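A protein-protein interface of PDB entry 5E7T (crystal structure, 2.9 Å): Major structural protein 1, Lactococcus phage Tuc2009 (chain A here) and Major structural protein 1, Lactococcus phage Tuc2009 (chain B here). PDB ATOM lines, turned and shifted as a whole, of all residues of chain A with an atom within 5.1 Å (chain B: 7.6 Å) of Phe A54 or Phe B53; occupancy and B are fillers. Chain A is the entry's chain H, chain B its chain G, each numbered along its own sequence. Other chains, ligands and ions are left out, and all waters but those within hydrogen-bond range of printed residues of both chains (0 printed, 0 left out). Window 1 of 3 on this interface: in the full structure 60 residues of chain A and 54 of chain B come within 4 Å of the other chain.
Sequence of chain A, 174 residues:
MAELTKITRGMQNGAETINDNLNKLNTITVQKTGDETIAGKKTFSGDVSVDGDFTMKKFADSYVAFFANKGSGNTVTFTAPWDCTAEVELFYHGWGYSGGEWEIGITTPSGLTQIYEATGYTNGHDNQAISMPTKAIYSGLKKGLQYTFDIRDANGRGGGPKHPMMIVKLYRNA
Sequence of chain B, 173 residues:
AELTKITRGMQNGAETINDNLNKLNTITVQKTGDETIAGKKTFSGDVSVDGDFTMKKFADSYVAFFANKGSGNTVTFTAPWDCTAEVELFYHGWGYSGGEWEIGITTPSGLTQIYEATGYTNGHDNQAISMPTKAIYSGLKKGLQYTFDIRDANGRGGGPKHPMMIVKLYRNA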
ATOM      1  N   VAL A  50       9.488 -18.618 -19.877  1.00  0.00           N
ATOM      2  CA  VAL A  50       9.661 -20.061 -19.652  1.00  0.00           C
ATOM      3  C   VAL A  50       8.300 -20.690 -19.273  1.00  0.00           C
ATOM      4  O   VAL A  50       7.847 -20.559 -18.128  1.00  0.00           O
ATOM      5  CB  VAL A  50      10.793 -20.406 -18.636  1.00  0.00           C
ATOM      6  CG1 VAL A  50      10.956 -21.916 -18.468  1.00  0.00           C
ATOM      7  CG2 VAL A  50      12.116 -19.772 -19.045  1.00  0.00           C
ATOM      8  N   GLY A  52       7.662 -23.959 -19.319  1.00  0.00           N
ATOM      9  CA  GLY A  52       7.961 -25.168 -18.563  1.00  0.00           C
ATOM     10  C   GLY A  52       8.486 -24.880 -17.178  1.00  0.00           C
ATOM     11  O   GLY A  52       8.249 -23.799 -16.626  1.00  0.00           O
ATOM     12  N   ASP A  53       9.216 -25.845 -16.617  1.00  0.00           N
ATOM     13  CA  ASP A  53       9.765 -25.723 -15.277  1.00  0.00           C
ATOM     14  C   ASP A  53      11.085 -24.965 -15.237  1.00  0.00           C
ATOM     15  O   ASP A  53      12.130 -25.518 -15.602  1.00  0.00           O
ATOM     16  CB  ASP A  53       9.875 -27.099 -14.597  1.00  0.00           C
ATOM     17  CG  ASP A  53       8.570 -27.608 -14.011  1.00  0.00           C
ATOM     18  OD1 ASP A  53       8.097 -27.016 -13.016  1.00  0.00           O
ATOM     19  OD2 ASP A  53       8.049 -28.629 -14.515  1.00  0.00           O
ATOM     20  N   PHE A  54      11.031 -23.688 -14.786  1.00  0.00           N
ATOM     21  CA  PHE A  54      12.218 -22.843 -14.630  1.00  0.00           C
ATOM     22  C   PHE A  54      12.968 -23.153 -13.338  1.00  0.00           C
ATOM     23  O   PHE A  54      12.406 -23.107 -12.235  1.00  0.00           O
ATOM     24  CB  PHE A  54      11.916 -21.338 -14.735  1.00  0.00           C
ATOM     25  CG  PHE A  54      13.172 -20.484 -14.756  1.00  0.00           C
ATOM     26  CD1 PHE A  54      13.986 -20.434 -15.889  1.00  0.00           C
ATOM     27  CD2 PHE A  54      13.541 -19.727 -13.647  1.00  0.00           C
ATOM     28  CE1 PHE A  54      15.150 -19.656 -15.901  1.00  0.00           C
ATOM     29  CE2 PHE A  54      14.698 -18.936 -13.671  1.00  0.00           C
ATOM     30  CZ  PHE A  54      15.498 -18.916 -14.793  1.00  0.00           C
ATOM     31  N   THR A  55      14.247 -23.463 -13.494  1.00  0.00           N
ATOM     32  CA  THR A  55      15.140 -23.796 -12.405  1.00  0.00           C
ATOM     33  C   THR A  55      16.248 -22.756 -12.414  1.00  0.00           C
ATOM     34  O   THR A  55      16.814 -22.449 -13.466  1.00  0.00           O
ATOM     35  CB  THR A  55      15.667 -25.233 -12.587  1.00  0.00           C
ATOM     36  OG1 THR A  55      14.580 -26.119 -12.874  1.00  0.00           O
ATOM     37  CG2 THR A  55      16.461 -25.736 -11.397  1.00  0.00           C
ATOM     38  N   MET A  56      16.512 -22.177 -11.244  1.00  0.00           N
ATOM     39  CA  MET A  56      17.592 -21.213 -11.020  1.00  0.00           C
ATOM     40  C   MET A  56      18.292 -21.595  -9.699  1.00  0.00           C
ATOM     41  O   MET A  56      17.633 -22.085  -8.771  1.00  0.00           O
ATOM     42  CB  MET A  56      17.096 -19.737 -11.043  1.00  0.00           C
ATOM     43  CG  MET A  56      16.200 -19.337  -9.871  1.00  0.00           C
ATOM     44  SD  MET A  56      15.674 -17.605  -9.808  1.00  0.00           S
ATOM     45  CE  MET A  56      13.928 -17.772 -10.191  1.00  0.00           C
ATOM     46  N   SER A  62      20.567 -14.383  -4.355  1.00  0.00           N
ATOM     47  CA  SER A  62      20.417 -13.590  -5.562  1.00  0.00           C
ATOM     48  C   SER A  62      19.354 -12.475  -5.472  1.00  0.00           C
ATOM     49  O   SER A  62      19.674 -11.337  -5.825  1.00  0.00           O
ATOM     50  CB  SER A  62      20.116 -14.520  -6.733  1.00  0.00           C
ATOM     51  OG  SER A  62      20.272 -13.909  -8.002  1.00  0.00           O
ATOM     52  N   TYR A  63      18.115 -12.770  -4.977  1.00  0.00           N
ATOM     53  CA  TYR A  63      17.012 -11.791  -4.985  1.00  0.00           C
ATOM     54  C   TYR A  63      16.501 -11.240  -3.625  1.00  0.00           C
ATOM     55  O   TYR A  63      15.798 -10.229  -3.667  1.00  0.00           O
ATOM     56  CB  TYR A  63      15.818 -12.336  -5.796  1.00  0.00           C
ATOM     57  CG  TYR A  63      16.187 -12.508  -7.254  1.00  0.00           C
ATOM     58  CD1 TYR A  63      16.167 -11.426  -8.131  1.00  0.00           C
ATOM     59  CD2 TYR A  63      16.676 -13.724  -7.732  1.00  0.00           C
ATOM     60  CE1 TYR A  63      16.602 -11.556  -9.451  1.00  0.00           C
ATOM     61  CE2 TYR A  63      17.086 -13.873  -9.058  1.00  0.00           C
ATOM     62  CZ  TYR A  63      17.047 -12.787  -9.915  1.00  0.00           C
ATOM     63  OH  TYR A  63      17.476 -12.930 -11.212  1.00  0.00           O
ATOM     64  N   PHE B  43      10.400 -20.150 -24.349  1.00  0.00           N
ATOM     65  CA  PHE B  43      10.787 -21.555 -24.185  1.00  0.00           C
ATOM     66  C   PHE B  43       9.580 -22.427 -23.792  1.00  0.00           C
ATOM     67  O   PHE B  43       8.992 -22.214 -22.730  1.00  0.00           O
ATOM     68  CB  PHE B  43      11.908 -21.701 -23.145  1.00  0.00           C
ATOM     69  CG  PHE B  43      13.250 -21.112 -23.516  1.00  0.00           C
ATOM     70  CD1 PHE B  43      13.559 -19.794 -23.203  1.00  0.00           C
ATOM     71  CD2 PHE B  43      14.233 -21.896 -24.106  1.00  0.00           C
ATOM     72  CE1 PHE B  43      14.816 -19.260 -23.510  1.00  0.00           C
ATOM     73  CE2 PHE B  43      15.496 -21.366 -24.395  1.00  0.00           C
ATOM     74  CZ  PHE B  43      15.780 -20.053 -24.094  1.00  0.00           C
ATOM     75  N   GLY B  45       9.484 -25.893 -23.221  1.00  0.00           N
ATOM     76  CA  GLY B  45       9.834 -26.860 -22.186  1.00  0.00           C
ATOM     77  C   GLY B  45      10.495 -26.284 -20.956  1.00  0.00           C
ATOM     78  O   GLY B  45      10.409 -25.079 -20.706  1.00  0.00           O
ATOM     79  N   ASP B  46      11.149 -27.154 -20.173  1.00  0.00           N
ATOM     80  CA  ASP B  46      11.847 -26.793 -18.937  1.00  0.00           C
ATOM     81  C   ASP B  46      13.152 -26.083 -19.243  1.00  0.00           C
ATOM     82  O   ASP B  46      13.789 -26.386 -20.249  1.00  0.00           O
ATOM     83  CB  ASP B  46      12.155 -28.056 -18.106  1.00  0.00           C
ATOM     84  CG  ASP B  46      10.964 -28.855 -17.599  1.00  0.00           C
ATOM     85  OD1 ASP B  46       9.807 -28.466 -17.900  1.00  0.00           O
ATOM     86  OD2 ASP B  46      11.187 -29.871 -16.902  1.00  0.00           O
ATOM     87  N   VAL B  47      13.559 -25.146 -18.374  1.00  0.00           N
ATOM     88  CA  VAL B  47      14.824 -24.401 -18.501  1.00  0.00           C
ATOM     89  C   VAL B  47      15.534 -24.426 -17.145  1.00  0.00           C
ATOM     90  O   VAL B  47      14.924 -24.092 -16.125  1.00  0.00           O
ATOM     91  CB  VAL B  47      14.638 -22.947 -19.034  1.00  0.00           C
ATOM     92  CG1 VAL B  47      15.931 -22.144 -18.934  1.00  0.00           C
ATOM     93  CG2 VAL B  47      14.119 -22.940 -20.465  1.00  0.00           C
ATOM     94  N   SER B  48      16.813 -24.827 -17.141  1.00  0.00           N
ATOM     95  CA  SER B  48      17.634 -24.870 -15.937  1.00  0.00           C
ATOM     96  C   SER B  48      18.921 -24.063 -16.158  1.00  0.00           C
ATOM     97  O   SER B  48      19.541 -24.161 -17.221  1.00  0.00           O
ATOM     98  CB  SER B  48      17.957 -26.309 -15.543  1.00  0.00           C
ATOM     99  OG  SER B  48      16.791 -27.046 -15.208  1.00  0.00           O
ATOM    100  N   VAL B  49      19.293 -23.235 -15.164  1.00  0.00           N
ATOM    101  CA  VAL B  49      20.501 -22.398 -15.188  1.00  0.00           C
ATOM    102  C   VAL B  49      21.413 -22.814 -14.015  1.00  0.00           C
ATOM    103  O   VAL B  49      21.134 -22.464 -12.857  1.00  0.00           O
ATOM    104  CB  VAL B  49      20.182 -20.878 -15.148  1.00  0.00           C
ATOM    105  CG1 VAL B  49      21.462 -20.055 -15.266  1.00  0.00           C
ATOM    106  CG2 VAL B  49      19.164 -20.475 -16.212  1.00  0.00           C
ATOM    107  N   ASP B  50      22.481 -23.576 -14.315  1.00  0.00           N
ATOM    108  CA  ASP B  50      23.460 -24.039 -13.324  1.00  0.00           C
ATOM    109  C   ASP B  50      24.330 -22.885 -12.793  1.00  0.00           C
ATOM    110  O   ASP B  50      24.708 -22.879 -11.617  1.00  0.00           O
ATOM    111  CB  ASP B  50      24.336 -25.169 -13.886  1.00  0.00           C
ATOM    112  CG  ASP B  50      23.579 -26.437 -14.264  1.00  0.00           C
ATOM    113  OD1 ASP B  50      22.447 -26.636 -13.746  1.00  0.00           O
ATOM    114  OD2 ASP B  50      24.123 -27.240 -15.067  1.00  0.00           O
ATOM    115  N   GLY B  51      24.603 -21.904 -13.651  1.00  0.00           N
ATOM    116  CA  GLY B  51      25.387 -20.728 -13.292  1.00  0.00           C
ATOM    117  C   GLY B  51      24.561 -19.648 -12.626  1.00  0.00           C
ATOM    118  O   GLY B  51      23.471 -19.916 -12.107  1.00  0.00           O
ATOM    119  N   ASP B  52      25.065 -18.419 -12.637  1.00  0.00           N
ATOM    120  CA  ASP B  52      24.362 -17.324 -11.979  1.00  0.00           C
ATOM    121  C   ASP B  52      23.214 -16.766 -12.815  1.00  0.00           C
ATOM    122  O   ASP B  52      23.455 -16.202 -13.886  1.00  0.00           O
ATOM    123  CB  ASP B  52      25.350 -16.216 -11.541  1.00  0.00           C
ATOM    124  CG  ASP B  52      26.541 -16.701 -10.724  1.00  0.00           C
ATOM    125  OD1 ASP B  52      26.610 -16.367  -9.524  1.00  0.00           O
ATOM    126  OD2 ASP B  52      27.413 -17.408 -11.295  1.00  0.00           O
ATOM    127  N   PHE B  53      21.967 -16.929 -12.345  1.00  0.00           N
ATOM    128  CA  PHE B  53      20.834 -16.343 -13.061  1.00  0.00           C
ATOM    129  C   PHE B  53      20.596 -14.879 -12.590  1.00  0.00           C
ATOM    130  O   PHE B  53      20.672 -14.598 -11.378  1.00  0.00           O
ATOM    131  CB  PHE B  53      19.567 -17.215 -12.989  1.00  0.00           C
ATOM    132  CG  PHE B  53      18.373 -16.618 -13.706  1.00  0.00           C
ATOM    133  CD1 PHE B  53      18.351 -16.516 -15.094  1.00  0.00           C
ATOM    134  CD2 PHE B  53      17.280 -16.142 -12.993  1.00  0.00           C
ATOM    135  CE1 PHE B  53      17.258 -15.936 -15.755  1.00  0.00           C
ATOM    136  CE2 PHE B  53      16.178 -15.581 -13.655  1.00  0.00           C
ATOM    137  CZ  PHE B  53      16.179 -15.474 -15.031  1.00  0.00           C
ATOM    138  N   THR B  54      20.359 -13.947 -13.564  1.00  0.00           N
ATOM    139  CA  THR B  54      20.150 -12.505 -13.339  1.00  0.00           C
ATOM    140  C   THR B  54      18.962 -11.969 -14.137  1.00  0.00           C
ATOM    141  O   THR B  54      18.909 -12.165 -15.355  1.00  0.00           O
ATOM    142  CB  THR B  54      21.416 -11.717 -13.711  1.00  0.00           C
ATOM    143  OG1 THR B  54      22.392 -12.606 -14.253  1.00  0.00           O
ATOM    144  CG2 THR B  54      21.996 -10.958 -12.535  1.00  0.00           C
ATOM    145  N   MET B  55      18.024 -11.271 -13.470  1.00  0.00           N
ATOM    146  CA  MET B  55      16.853 -10.713 -14.162  1.00  0.00           C
ATOM    147  C   MET B  55      16.550  -9.257 -13.758  1.00  0.00           C
ATOM    148  O   MET B  55      16.981  -8.785 -12.697  1.00  0.00           O
ATOM    149  CB  MET B  55      15.603 -11.624 -14.015  1.00  0.00           C
ATOM    150  CG  MET B  55      14.899 -11.532 -12.653  1.00  0.00           C
ATOM    151  SD  MET B  55      13.997 -13.026 -12.111  1.00  0.00           S
ATOM    152  CE  MET B  55      12.416 -12.631 -12.708  1.00  0.00           C
ATOM    153  N   LYS B  56      15.797  -8.561 -14.633  1.00  0.00           N
ATOM    154  CA  LYS B  56      15.372  -7.169 -14.464  1.00  0.00           C
ATOM    155  C   LYS B  56      13.980  -7.098 -13.825  1.00  0.00           C
ATOM    156  O   LYS B  56      13.193  -8.041 -13.969  1.00  0.00           O
ATOM    157  CB  LYS B  56      15.368  -6.441 -15.826  1.00  0.00           C
ATOM    158  CG  LYS B  56      16.387  -5.317 -15.953  1.00  0.00           C
ATOM    159  CD  LYS B  56      17.738  -5.809 -16.460  1.00  0.00           C
ATOM    160  CE  LYS B  56      18.636  -4.673 -16.893  1.00  0.00           C
ATOM    161  NZ  LYS B  56      19.872  -5.167 -17.559  1.00  0.00           N
ATOM    162  N   PHE B  58      12.398  -7.621 -10.936  1.00  0.00           N
ATOM    163  CA  PHE B  58      11.784  -8.797 -10.306  1.00  0.00           C
ATOM    164  C   PHE B  58      10.640  -8.414  -9.364  1.00  0.00           C
ATOM    165  O   PHE B  58       9.538  -8.957  -9.472  1.00  0.00           O
ATOM    166  CB  PHE B  58      12.815  -9.693  -9.565  1.00  0.00           C
ATOM    167  CG  PHE B  58      12.160 -10.725  -8.659  1.00  0.00           C
ATOM    168  CD1 PHE B  58      11.694 -11.934  -9.175  1.00  0.00           C
ATOM    169  CD2 PHE B  58      11.939 -10.455  -7.308  1.00  0.00           C
ATOM    170  CE1 PHE B  58      11.034 -12.857  -8.353  1.00  0.00           C
ATOM    171  CE2 PHE B  58      11.261 -11.370  -6.495  1.00  0.00           C
ATOM    172  CZ  PHE B  58      10.826 -12.568  -7.020  1.00  0.00           C
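The backbone carbonyl oxygen of Gly B45 sits close to the backbone NH of Gly A52, at 3.3 Å.
The backbone NH of Asp A53 sits at hydrogen-bond distance from the side-chain carboxylate of Asp B46 (3.0 Å).
N of Val B47 sits at hydrogen-bond distance from O of Asp A53 (3.1 Å).
O of Val B47 lies within hydrogen-bond range of N of Thr A55 (2.8 Å).
The side-chain hydroxyl (OG1) of Thr A55 lies within hydrogen-bond range of the side-chain hydroxyl (OG) of Ser B48 (3.3 Å).
The backbone NH (N) of Val B49 sits at hydrogen-bond distance from the backbone carbonyl oxygen (O) of Thr A55.
O of Phe B53 lies within hydrogen-bond range of OG of Ser A62 (3.5 Å).
The backbone NH of Met B55 lies within hydrogen-bond range of the side-chain hydroxyl of Tyr A63 (2.9 Å).
Val A50 touches Phe B43 (CA to O, 3.8 Å).
Val A50 touches Gly B45.
CG1 of Val A50 touches CB of Val B47, at 3.9 Å.
CA of Gly A52 touches OD1 of Asp B46, 3.8 Å away.
Phe A54 touches Val B47 (CA to O, 3.3 Å).
Phe A54 touches Phe B53 (CZ to CZ, 3.5 Å).
Met A56 touches Phe B53.
Phe B53 touches Tyr A63 (O to OH, 3.6 Å).
C of Thr B54 touches OH of Tyr A63 (3.4 Å).
Of the printed residues of chain B, Phe A54 touches Val B47 and Phe B53.
Of the printed residues of chain B, Ser A62 touches Phe B53.
Phe B53 touches just these residues of chain A: Phe A54 (3.5 Å), Met A56 (3.9 Å), Ser A62 (3.5 Å) and Tyr A63 (3.6 Å).
Of the printed residues of chain A, Met B55 touches Tyr A63.
The nearest printed residue of chain A that does not touch Phe B53 is Thr A55 (5.9 Å).
Printed residues of chain B that touch a printed residue of chain A: Phe B43, Gly B45, Asp B46, Val B47, Ser B48, Val B49, Phe B53, Thr B54 and Met B55.
Hydrophobic or aromatic side chains of chain B that line the printed part of chain A: Val B47, Phe B53 and Met B55.
Of the 8 printed residues of chain A, 8 touch a printed residue of chain B.
Hydrophobic or aromatic side chains of chain A within 4 Å of the printed part of chain B: Val A50, Phe A54, Met A56 and Tyr A63.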
